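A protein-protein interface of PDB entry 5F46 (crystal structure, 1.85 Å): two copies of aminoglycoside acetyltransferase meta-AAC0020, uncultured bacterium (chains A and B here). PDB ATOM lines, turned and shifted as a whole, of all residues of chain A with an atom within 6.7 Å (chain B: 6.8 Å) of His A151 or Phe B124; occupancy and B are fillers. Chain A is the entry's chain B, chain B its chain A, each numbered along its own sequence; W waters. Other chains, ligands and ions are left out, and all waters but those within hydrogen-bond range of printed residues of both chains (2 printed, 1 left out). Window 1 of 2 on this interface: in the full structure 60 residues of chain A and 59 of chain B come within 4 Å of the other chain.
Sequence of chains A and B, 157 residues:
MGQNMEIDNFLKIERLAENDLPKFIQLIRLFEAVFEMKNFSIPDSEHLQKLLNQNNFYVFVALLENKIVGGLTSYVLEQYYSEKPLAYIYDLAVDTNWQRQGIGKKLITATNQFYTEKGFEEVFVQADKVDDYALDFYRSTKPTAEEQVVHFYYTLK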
ATOM      1  N   TYR A  88       4.136   7.705  -5.113  1.00  0.00           N
ATOM      2  CA  TYR A  88       4.366   7.803  -3.680  1.00  0.00           C
ATOM      3  C   TYR A  88       3.026   7.781  -2.949  1.00  0.00           C
ATOM      4  O   TYR A  88       2.251   8.721  -3.083  1.00  0.00           O
ATOM      5  CB  TYR A  88       5.122   9.097  -3.366  1.00  0.00           C
ATOM      6  CG  TYR A  88       5.422   9.354  -1.907  1.00  0.00           C
ATOM      7  CD1 TYR A  88       5.515   8.315  -0.994  1.00  0.00           C
ATOM      8  CD2 TYR A  88       5.610  10.651  -1.444  1.00  0.00           C
ATOM      9  CE1 TYR A  88       5.798   8.558   0.336  1.00  0.00           C
ATOM     10  CE2 TYR A  88       5.886  10.903  -0.116  1.00  0.00           C
ATOM     11  CZ  TYR A  88       5.978   9.853   0.770  1.00  0.00           C
ATOM     12  OH  TYR A  88       6.257  10.102   2.093  1.00  0.00           O
ATOM     13  N   TYR A  90       1.126   8.557   0.113  1.00  0.00           N
ATOM     14  CA  TYR A  90       1.414   9.476   1.204  1.00  0.00           C
ATOM     15  C   TYR A  90       0.675   9.105   2.484  1.00  0.00           C
ATOM     16  O   TYR A  90       1.289   8.977   3.543  1.00  0.00           O
ATOM     17  CB  TYR A  90       1.068  10.912   0.809  1.00  0.00           C
ATOM     18  CG  TYR A  90       1.488  11.905   1.859  1.00  0.00           C
ATOM     19  CD1 TYR A  90       2.791  12.388   1.901  1.00  0.00           C
ATOM     20  CD2 TYR A  90       0.592  12.340   2.829  1.00  0.00           C
ATOM     21  CE1 TYR A  90       3.184  13.287   2.871  1.00  0.00           C
ATOM     22  CE2 TYR A  90       0.977  13.233   3.804  1.00  0.00           C
ATOM     23  CZ  TYR A  90       2.272  13.705   3.819  1.00  0.00           C
ATOM     24  OH  TYR A  90       2.654  14.597   4.790  1.00  0.00           O
ATOM     25  N   GLN A 126       5.680   4.679   3.248  1.00  0.00           N
ATOM     26  CA  GLN A 126       6.415   4.619   4.480  1.00  0.00           C
ATOM     27  C   GLN A 126       5.534   4.407   5.692  1.00  0.00           C
ATOM     28  O   GLN A 126       4.369   4.757   5.695  1.00  0.00           O
ATOM     29  CB  GLN A 126       7.246   5.854   4.699  1.00  0.00           C
ATOM     30  CG  GLN A 126       6.423   7.057   5.108  1.00  0.00           C
ATOM     31  CD  GLN A 126       6.734   7.611   6.481  1.00  0.00           C
ATOM     32  OE1 GLN A 126       7.401   8.627   6.603  1.00  0.00           O
ATOM     33  NE2 GLN A 126       6.203   6.971   7.518  1.00  0.00           N
ATOM     34  N   VAL A 149      14.877   3.383   7.402  1.00  0.00           N
ATOM     35  CA  VAL A 149      15.282   4.734   7.043  1.00  0.00           C
ATOM     36  C   VAL A 149      14.993   5.741   8.153  1.00  0.00           C
ATOM     37  O   VAL A 149      14.284   5.444   9.116  1.00  0.00           O
ATOM     38  CB  VAL A 149      14.585   5.208   5.751  1.00  0.00           C
ATOM     39  CG1 VAL A 149      15.233   4.585   4.523  1.00  0.00           C
ATOM     40  CG2 VAL A 149      13.102   4.886   5.798  1.00  0.00           C
ATOM     41  N   VAL A 150      15.556   6.934   8.010  1.00  0.00           N
ATOM     42  CA  VAL A 150      15.305   8.011   8.955  1.00  0.00           C
ATOM     43  C   VAL A 150      14.709   9.205   8.217  1.00  0.00           C
ATOM     44  O   VAL A 150      15.282   9.699   7.246  1.00  0.00           O
ATOM     45  CB  VAL A 150      16.588   8.436   9.694  1.00  0.00           C
ATOM     46  CG1 VAL A 150      16.285   9.530  10.705  1.00  0.00           C
ATOM     47  CG2 VAL A 150      17.221   7.238  10.386  1.00  0.00           C
ATOM     48  N   HIS A 151      13.549   9.651   8.684  1.00  0.00           N
ATOM     49  CA  HIS A 151      12.836  10.776   8.093  1.00  0.00           C
ATOM     50  C   HIS A 151      13.190  12.068   8.827  1.00  0.00           C
ATOM     51  O   HIS A 151      13.015  12.167  10.042  1.00  0.00           O
ATOM     52  CB  HIS A 151      11.326  10.507   8.134  1.00  0.00           C
ATOM     53  CG  HIS A 151      10.476  11.675   7.748  1.00  0.00           C
ATOM     54  ND1 HIS A 151       9.820  12.458   8.677  1.00  0.00           N
ATOM     55  CD2 HIS A 151      10.148  12.181   6.536  1.00  0.00           C
ATOM     56  CE1 HIS A 151       9.138  13.401   8.054  1.00  0.00           C
ATOM     57  NE2 HIS A 151       9.319  13.255   6.752  1.00  0.00           N
ATOM     58  N   PHE A 152      13.720  13.038   8.087  1.00  0.00           N
ATOM     59  CA  PHE A 152      14.013  14.361   8.631  1.00  0.00           C
ATOM     60  C   PHE A 152      13.048  15.377   8.055  1.00  0.00           C
ATOM     61  O   PHE A 152      12.747  15.332   6.864  1.00  0.00           O
ATOM     62  CB  PHE A 152      15.446  14.792   8.311  1.00  0.00           C
ATOM     63  CG  PHE A 152      16.501  13.878   8.863  1.00  0.00           C
ATOM     64  CD1 PHE A 152      17.008  14.080  10.133  1.00  0.00           C
ATOM     65  CD2 PHE A 152      17.002  12.833   8.103  1.00  0.00           C
ATOM     66  CE1 PHE A 152      17.986  13.247  10.648  1.00  0.00           C
ATOM     67  CE2 PHE A 152      17.979  11.999   8.608  1.00  0.00           C
ATOM     68  CZ  PHE A 152      18.472  12.205   9.884  1.00  0.00           C
ATOM     69  N   TYR A 153      12.560  16.301   8.875  1.00  0.00           N
ATOM     70  CA  TYR A 153      11.757  17.375   8.311  1.00  0.00           C
ATOM     71  C   TYR A 153      12.056  18.731   8.937  1.00  0.00           C
ATOM     72  O   TYR A 153      12.528  18.836  10.076  1.00  0.00           O
ATOM     73  CB  TYR A 153      10.261  17.045   8.406  1.00  0.00           C
ATOM     74  CG  TYR A 153       9.664  17.055   9.792  1.00  0.00           C
ATOM     75  CD1 TYR A 153       9.146  18.225  10.338  1.00  0.00           C
ATOM     76  CD2 TYR A 153       9.579  15.890  10.540  1.00  0.00           C
ATOM     77  CE1 TYR A 153       8.584  18.239  11.599  1.00  0.00           C
ATOM     78  CE2 TYR A 153       9.017  15.893  11.805  1.00  0.00           C
ATOM     79  CZ  TYR A 153       8.521  17.071  12.329  1.00  0.00           C
ATOM     80  OH  TYR A 153       7.961  17.086  13.585  1.00  0.00           O
ATOM     81  N   TYR A 154      11.799  19.764   8.146  1.00  0.00           N
ATOM     82  CA  TYR A 154      12.093  21.138   8.511  1.00  0.00           C
ATOM     83  C   TYR A 154      10.810  21.947   8.481  1.00  0.00           C
ATOM     84  O   TYR A 154      10.280  22.227   7.411  1.00  0.00           O
ATOM     85  CB  TYR A 154      13.115  21.754   7.546  1.00  0.00           C
ATOM     86  CG  TYR A 154      14.382  20.944   7.344  1.00  0.00           C
ATOM     87  CD1 TYR A 154      14.416  19.868   6.463  1.00  0.00           C
ATOM     88  CD2 TYR A 154      15.550  21.273   8.016  1.00  0.00           C
ATOM     89  CE1 TYR A 154      15.580  19.130   6.269  1.00  0.00           C
ATOM     90  CE2 TYR A 154      16.716  20.542   7.832  1.00  0.00           C
ATOM     91  CZ  TYR A 154      16.725  19.475   6.958  1.00  0.00           C
ATOM     92  OH  TYR A 154      17.885  18.752   6.780  1.00  0.00           O
ATOM     93  N   TYR B  75      10.675  17.722  -4.930  1.00  0.00           N
ATOM     94  CA  TYR B  75       9.343  17.667  -5.514  1.00  0.00           C
ATOM     95  C   TYR B  75       8.348  18.407  -4.639  1.00  0.00           C
ATOM     96  O   TYR B  75       8.401  18.314  -3.415  1.00  0.00           O
ATOM     97  CB  TYR B  75       8.873  16.222  -5.681  1.00  0.00           C
ATOM     98  CG  TYR B  75       9.636  15.413  -6.702  1.00  0.00           C
ATOM     99  CD1 TYR B  75      10.795  14.736  -6.356  1.00  0.00           C
ATOM    100  CD2 TYR B  75       9.175  15.306  -8.006  1.00  0.00           C
ATOM    101  CE1 TYR B  75      11.494  13.981  -7.295  1.00  0.00           C
ATOM    102  CE2 TYR B  75       9.861  14.553  -8.951  1.00  0.00           C
ATOM    103  CZ  TYR B  75      11.021  13.897  -8.588  1.00  0.00           C
ATOM    104  OH  TYR B  75      11.700  13.145  -9.524  1.00  0.00           O
ATOM    105  N   LEU B  77       4.704  18.729  -3.146  1.00  0.00           N
ATOM    106  CA  LEU B  77       3.523  17.926  -2.862  1.00  0.00           C
ATOM    107  C   LEU B  77       2.445  18.841  -2.300  1.00  0.00           C
ATOM    108  O   LEU B  77       2.499  19.215  -1.128  1.00  0.00           O
ATOM    109  CB  LEU B  77       3.842  16.803  -1.869  1.00  0.00           C
ATOM    110  CG  LEU B  77       5.021  15.883  -2.202  1.00  0.00           C
ATOM    111  CD1 LEU B  77       5.153  14.804  -1.141  1.00  0.00           C
ATOM    112  CD2 LEU B  77       4.869  15.261  -3.584  1.00  0.00           C
ATOM    113  N   LEU B  86       3.940  20.863   0.701  1.00  0.00           N
ATOM    114  CA  LEU B  86       5.149  20.210   1.181  1.00  0.00           C
ATOM    115  C   LEU B  86       6.174  20.164   0.066  1.00  0.00           C
ATOM    116  O   LEU B  86       5.817  20.161  -1.114  1.00  0.00           O
ATOM    117  CB  LEU B  86       4.855  18.788   1.652  1.00  0.00           C
ATOM    118  CG  LEU B  86       3.767  18.632   2.712  1.00  0.00           C
ATOM    119  CD1 LEU B  86       3.432  17.162   2.898  1.00  0.00           C
ATOM    120  CD2 LEU B  86       4.192  19.265   4.025  1.00  0.00           C
ATOM    121  N   ALA B  87       7.446  20.118   0.444  1.00  0.00           N
ATOM    122  CA  ALA B  87       8.505  19.823  -0.509  1.00  0.00           C
ATOM    123  C   ALA B  87       9.247  18.572  -0.056  1.00  0.00           C
ATOM    124  O   ALA B  87       9.559  18.409   1.126  1.00  0.00           O
ATOM    125  CB  ALA B  87       9.455  20.994  -0.652  1.00  0.00           C
ATOM    126  N   TYR B  88       9.502  17.688  -1.008  1.00  0.00           N
ATOM    127  CA  TYR B  88      10.178  16.428  -0.752  1.00  0.00           C
ATOM    128  C   TYR B  88      11.536  16.450  -1.441  1.00  0.00           C
ATOM    129  O   TYR B  88      11.598  16.476  -2.666  1.00  0.00           O
ATOM    130  CB  TYR B  88       9.327  15.268  -1.273  1.00  0.00           C
ATOM    131  CG  TYR B  88       9.919  13.886  -1.099  1.00  0.00           C
ATOM    132  CD1 TYR B  88      10.792  13.596  -0.057  1.00  0.00           C
ATOM    133  CD2 TYR B  88       9.607  12.869  -1.993  1.00  0.00           C
ATOM    134  CE1 TYR B  88      11.329  12.322   0.096  1.00  0.00           C
ATOM    135  CE2 TYR B  88      10.137  11.600  -1.850  1.00  0.00           C
ATOM    136  CZ  TYR B  88      10.996  11.332  -0.804  1.00  0.00           C
ATOM    137  OH  TYR B  88      11.522  10.068  -0.663  1.00  0.00           O
ATOM    138  N   ILE B  89      12.615  16.468  -0.661  1.00  0.00           N
ATOM    139  CA  ILE B  89      13.956  16.336  -1.226  1.00  0.00           C
ATOM    140  C   ILE B  89      14.203  14.862  -1.499  1.00  0.00           C
ATOM    141  O   ILE B  89      14.196  14.048  -0.577  1.00  0.00           O
ATOM    142  CB  ILE B  89      15.050  16.886  -0.288  1.00  0.00           C
ATOM    143  CG1 ILE B  89      14.795  18.368   0.004  1.00  0.00           C
ATOM    144  CG2 ILE B  89      16.451  16.659  -0.905  1.00  0.00           C
ATOM    145  CD1 ILE B  89      15.740  18.974   1.037  1.00  0.00           C
ATOM    146  N   TYR B  90      14.407  14.523  -2.764  1.00  0.00           N
ATOM    147  CA  TYR B  90      14.484  13.125  -3.164  1.00  0.00           C
ATOM    148  C   TYR B  90      15.918  12.614  -3.171  1.00  0.00           C
ATOM    149  O   TYR B  90      16.224  11.600  -2.541  1.00  0.00           O
ATOM    150  CB  TYR B  90      13.845  12.933  -4.538  1.00  0.00           C
ATOM    151  CG  TYR B  90      13.807  11.488  -4.980  1.00  0.00           C
ATOM    152  CD1 TYR B  90      12.768  10.651  -4.596  1.00  0.00           C
ATOM    153  CD2 TYR B  90      14.825  10.957  -5.764  1.00  0.00           C
ATOM    154  CE1 TYR B  90      12.736   9.325  -4.998  1.00  0.00           C
ATOM    155  CE2 TYR B  90      14.804   9.638  -6.165  1.00  0.00           C
ATOM    156  CZ  TYR B  90      13.761   8.826  -5.778  1.00  0.00           C
ATOM    157  OH  TYR B  90      13.744   7.511  -6.182  1.00  0.00           O
ATOM    158  N   ASN B 112      15.473  25.307   1.706  1.00  0.00           N
ATOM    159  CA  ASN B 112      14.460  25.641   2.697  1.00  0.00           C
ATOM    160  C   ASN B 112      14.053  27.110   2.626  1.00  0.00           C
ATOM    161  O   ASN B 112      12.896  27.450   2.873  1.00  0.00           O
ATOM    162  CB  ASN B 112      14.948  25.287   4.102  1.00  0.00           C
ATOM    163  CG  ASN B 112      15.003  23.787   4.332  1.00  0.00           C
ATOM    164  OD1 ASN B 112      14.473  23.011   3.535  1.00  0.00           O
ATOM    165  ND2 ASN B 112      15.642  23.372   5.417  1.00  0.00           N
ATOM    166  N   GLU B 122       6.489  22.824   5.106  1.00  0.00           N
ATOM    167  CA  GLU B 122       7.507  21.882   5.552  1.00  0.00           C
ATOM    168  C   GLU B 122       8.302  21.288   4.389  1.00  0.00           C
ATOM    169  O   GLU B 122       7.762  21.036   3.310  1.00  0.00           O
ATOM    170  CB  GLU B 122       6.830  20.774   6.367  1.00  0.00           C
ATOM    171  CG  GLU B 122       7.661  19.550   6.686  1.00  0.00           C
ATOM    172  CD  GLU B 122       6.843  18.489   7.409  1.00  0.00           C
ATOM    173  OE1 GLU B 122       6.760  17.347   6.908  1.00  0.00           O
ATOM    174  OE2 GLU B 122       6.275  18.802   8.478  1.00  0.00           O
ATOM    175  N   VAL B 123       9.592  21.085   4.622  1.00  0.00           N
ATOM    176  CA  VAL B 123      10.455  20.338   3.709  1.00  0.00           C
ATOM    177  C   VAL B 123      10.916  19.075   4.427  1.00  0.00           C
ATOM    178  O   VAL B 123      11.294  19.133   5.593  1.00  0.00           O
ATOM    179  CB  VAL B 123      11.680  21.171   3.264  1.00  0.00           C
ATOM    180  CG1 VAL B 123      12.604  20.344   2.380  1.00  0.00           C
ATOM    181  CG2 VAL B 123      11.238  22.433   2.536  1.00  0.00           C
ATOM    182  N   PHE B 124      10.872  17.928   3.758  1.00  0.00           N
ATOM    183  CA  PHE B 124      11.392  16.715   4.382  1.00  0.00           C
ATOM    184  C   PHE B 124      12.276  15.904   3.441  1.00  0.00           C
ATOM    185  O   PHE B 124      12.319  16.147   2.233  1.00  0.00           O
ATOM    186  CB  PHE B 124      10.251  15.846   4.922  1.00  0.00           C
ATOM    187  CG  PHE B 124       9.333  15.298   3.862  1.00  0.00           C
ATOM    188  CD1 PHE B 124       8.286  16.062   3.369  1.00  0.00           C
ATOM    189  CD2 PHE B 124       9.499  14.008   3.379  1.00  0.00           C
ATOM    190  CE1 PHE B 124       7.434  15.555   2.396  1.00  0.00           C
ATOM    191  CE2 PHE B 124       8.648  13.494   2.410  1.00  0.00           C
ATOM    192  CZ  PHE B 124       7.619  14.267   1.915  1.00  0.00           C
ATOM    193  N   VAL B 125      12.985  14.938   4.014  1.00  0.00           N
ATOM    194  CA  VAL B 125      14.009  14.196   3.288  1.00  0.00           C
ATOM    195  C   VAL B 125      14.326  12.902   4.041  1.00  0.00           C
ATOM    196  O   VAL B 125      14.227  12.859   5.270  1.00  0.00           O
ATOM    197  CB  VAL B 125      15.285  15.056   3.102  1.00  0.00           C
ATOM    198  CG1 VAL B 125      15.821  15.528   4.447  1.00  0.00           C
ATOM    199  CG2 VAL B 125      16.357  14.307   2.299  1.00  0.00           C
ATOM    200  N   GLN B 126      14.680  11.847   3.310  1.00  0.00           N
ATOM    201  CA  GLN B 126      15.006  10.568   3.935  1.00  0.00           C
ATOM    202  C   GLN B 126      16.477  10.205   3.756  1.00  0.00           C
ATOM    203  O   GLN B 126      17.104  10.539   2.745  1.00  0.00           O
ATOM    204  CB  GLN B 126      14.124   9.443   3.377  1.00  0.00           C
ATOM    205  CG  GLN B 126      14.405   9.063   1.923  1.00  0.00           C
ATOM    206  CD  GLN B 126      14.219   7.576   1.645  1.00  0.00           C
ATOM    207  OE1 GLN B 126      13.134   7.027   1.835  1.00  0.00           O
ATOM    208  NE2 GLN B 126      15.283   6.921   1.191  1.00  0.00           N
ATOM    209  N   ALA B 127      17.027   9.520   4.752  1.00  0.00           N
ATOM    210  CA  ALA B 127      18.372   8.972   4.648  1.00  0.00           C
ATOM    211  C   ALA B 127      18.371   7.541   5.164  1.00  0.00           C
ATOM    212  O   ALA B 127      17.611   7.196   6.070  1.00  0.00           O
ATOM    213  CB  ALA B 127      19.367   9.822   5.416  1.00  0.00           C
ATOM    214  N   LEU B 135      23.407  10.464   7.492  1.00  0.00           N
ATOM    215  CA  LEU B 135      22.638  10.512   8.730  1.00  0.00           C
ATOM    216  C   LEU B 135      23.137  11.600   9.676  1.00  0.00           C
ATOM    217  O   LEU B 135      22.343  12.274  10.332  1.00  0.00           O
ATOM    218  CB  LEU B 135      22.685   9.155   9.427  1.00  0.00           C
ATOM    219  CG  LEU B 135      21.382   8.675  10.056  1.00  0.00           C
ATOM    220  CD1 LEU B 135      20.243   8.838   9.066  1.00  0.00           C
ATOM    221  CD2 LEU B 135      21.521   7.224  10.482  1.00  0.00           C
ATOM    222  N   ALA B 145      12.718  18.016  13.323  1.00  0.00           N
ATOM    223  CA  ALA B 145      12.656  16.717  13.979  1.00  0.00           C
ATOM    224  C   ALA B 145      13.109  15.604  13.051  1.00  0.00           C
ATOM    225  O   ALA B 145      13.175  15.777  11.835  1.00  0.00           O
ATOM    226  CB  ALA B 145      11.246  16.440  14.481  1.00  0.00           C
ATOM    227  N   GLU B 146      13.428  14.460  13.644  1.00  0.00           N
ATOM    228  CA  GLU B 146      13.758  13.268  12.880  1.00  0.00           C
ATOM    229  C   GLU B 146      12.973  12.081  13.418  1.00  0.00           C
ATOM    230  O   GLU B 146      12.712  11.986  14.617  1.00  0.00           O
ATOM    231  CB  GLU B 146      15.259  12.979  12.922  1.00  0.00           C
ATOM    232  CG  GLU B 146      15.786  12.554  14.279  1.00  0.00           C
ATOM    233  CD  GLU B 146      17.162  11.933  14.186  1.00  0.00           C
ATOM    234  OE1 GLU B 146      17.247  10.688  14.092  1.00  0.00           O
ATOM    235  OE2 GLU B 146      18.158  12.687  14.206  1.00  0.00           O
ATOM    236  N   GLU B 147      12.583  11.186  12.522  1.00  0.00           N
ATOM    237  CA  GLU B 147      11.782  10.031  12.889  1.00  0.00           C
ATOM    238  C   GLU B 147      12.288   8.769  12.217  1.00  0.00           C
ATOM    239  O   GLU B 147      12.480   8.738  11.004  1.00  0.00           O
ATOM    240  CB  GLU B 147      10.313  10.254  12.520  1.00  0.00           C
ATOM    241  CG  GLU B 147       9.654  11.407  13.253  1.00  0.00           C
ATOM    242  CD  GLU B 147       9.421  11.100  14.720  1.00  0.00           C
ATOM    243  OE1 GLU B 147       9.361   9.903  15.078  1.00  0.00           O
ATOM    244  OE2 GLU B 147       9.303  12.054  15.519  1.00  0.00           O
ATOM    245  N   GLN B 148      12.499   7.725  13.008  1.00  0.00           N
ATOM    246  CA  GLN B 148      12.853   6.437  12.440  1.00  0.00           C
ATOM    247  C   GLN B 148      11.638   5.835  11.750  1.00  0.00           C
ATOM    248  O   GLN B 148      10.575   5.696  12.354  1.00  0.00           O
ATOM    249  CB  GLN B 148      13.385   5.495  13.518  1.00  0.00           C
ATOM    250  CG  GLN B 148      14.559   6.045  14.303  1.00  0.00           C
ATOM    251  CD  GLN B 148      15.884   5.779  13.620  1.00  0.00           C
ATOM    252  OE1 GLN B 148      15.953   5.010  12.663  1.00  0.00           O
ATOM    253  NE2 GLN B 148      16.949   6.398  14.120  1.00  0.00           N
ATOM    254  N   VAL B 149      11.788   5.495  10.474  1.00  0.00           N
ATOM    255  CA  VAL B 149      10.676   4.925   9.720  1.00  0.00           C
ATOM    256  C   VAL B 149      11.109   3.757   8.835  1.00  0.00           C
ATOM    257  O   VAL B 149      12.300   3.503   8.656  1.00  0.00           O
ATOM    258  CB  VAL B 149       9.990   5.990   8.834  1.00  0.00           C
ATOM    259  CG1 VAL B 149       9.180   6.963   9.683  1.00  0.00           C
ATOM    260  CG2 VAL B 149      11.009   6.726   7.985  1.00  0.00           C
HETATM  261  O   HOH W   1       7.329  14.507  15.005  1.00  0.00           O
HETATM  262  O   HOH W   2      13.352   2.619  10.684  1.00  0.00           O
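The backbone carbonyl oxygen of His A151 sits at hydrogen-bond distance from the backbone NH of Glu B147, 2.7 Å away.
The backbone carbonyl oxygen (O) of Val B125 sits at hydrogen-bond distance from the backbone NH (N) of Phe A152 (2.9 Å).
The backbone NH of Val A150 is in hydrogen-bond range of the backbone carbonyl oxygen of Ala B127, at 2.8 Å.
The backbone NH of Tyr A154 sits at hydrogen-bond distance from the backbone carbonyl oxygen of Val B123, at 2.7 Å.
The backbone carbonyl oxygen of Ala B145 lies within hydrogen-bond range of the backbone NH of Tyr A153, at 3.1 Å.
The backbone carbonyl oxygen of Val A149 lies within hydrogen-bond range of the backbone NH of Val B149 (2.8 Å).
Of the printed residues of chain A, Phe B124 touches His A151 (3.3 Å), Phe A152 (3.1 Å) and Tyr A153 (3.7 Å).
Of the printed residues of chain A, Ala B127 touches Val A149 (3.5 Å) and Val A150 (2.8 Å).
Printed residues of chain B within 4 Å of Phe A152: Phe B124, Val B125, Leu B135, Ala B145 and Glu B146.
Of the printed residues of chain A, Glu B146 touches Val A150 (3.7 Å), His A151 (3.1 Å) and Phe A152 (3.5 Å).
Among the printed residues, 29 pairs touch across the chains.
Among the printed residues, no Asp or Glu carboxylate lies within 4 Å of a Lys or Arg side-chain nitrogen of the other chain.
Among the printed residues, pairs that only touch across the chains: Tyr A90 with Leu B86, Gln A126 with Val B149, Val A149 with Ala B127, Val A149 with Gln B148, Val A150 with Val B125, Val A150 with Gln B126, Val A150 with Leu B135, Val A150 with Glu B146, Val A150 with Glu B147, Val A150 with Gln B148, His A151 with Phe B124, His A151 with Val B125, His A151 with Glu B146, His A151 with Val B149, Phe A152 with Phe B124, Phe A152 with Leu B135, Phe A152 with Ala B145, Phe A152 with Glu B146, Tyr A153 with Glu B122, Tyr A153 with Val B123, Tyr A153 with Phe B124, Tyr A154 with Asn B112 and Tyr A154 with Glu B122.
The backbone carbonyl oxygen of Leu B86 lies within hydrogen-bond range of the backbone NH of Leu B77 (2.7 Å).
The backbone NH (N) of Ile B89 is in hydrogen-bond range of the backbone carbonyl oxygen (O) of Phe B124 (2.9 Å).
The backbone carbonyl oxygen (O) of Ala B87 sits at hydrogen-bond distance from the backbone NH (N) of Phe B124, at 3.0 Å.
The backbone NH (N) of Ala B87 lies within hydrogen-bond range of the backbone carbonyl oxygen (O) of Glu B122, 3.0 Å away.
Water W2 bridges the backbone carbonyl oxygen of Val B149 (2.4 Å) and the backbone carbonyl oxygen of Val A149 (3.4 Å).
Water W1 lies within hydrogen-bond range of the side-chain hydroxyl of Tyr A153 (3.0 Å) and the side-chain carboxylate of Glu B147 (3.2 Å).
Gln A126 touches Val B149, but with the chains exchanged Val A149 does not touch Gln B126 (4.1 Å).
Val B149 touches its own counterpart, Val A149.
Of the 29 pairs that touch across the chains among the printed residues, 1 has its exchanged pair printed and touching as well.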
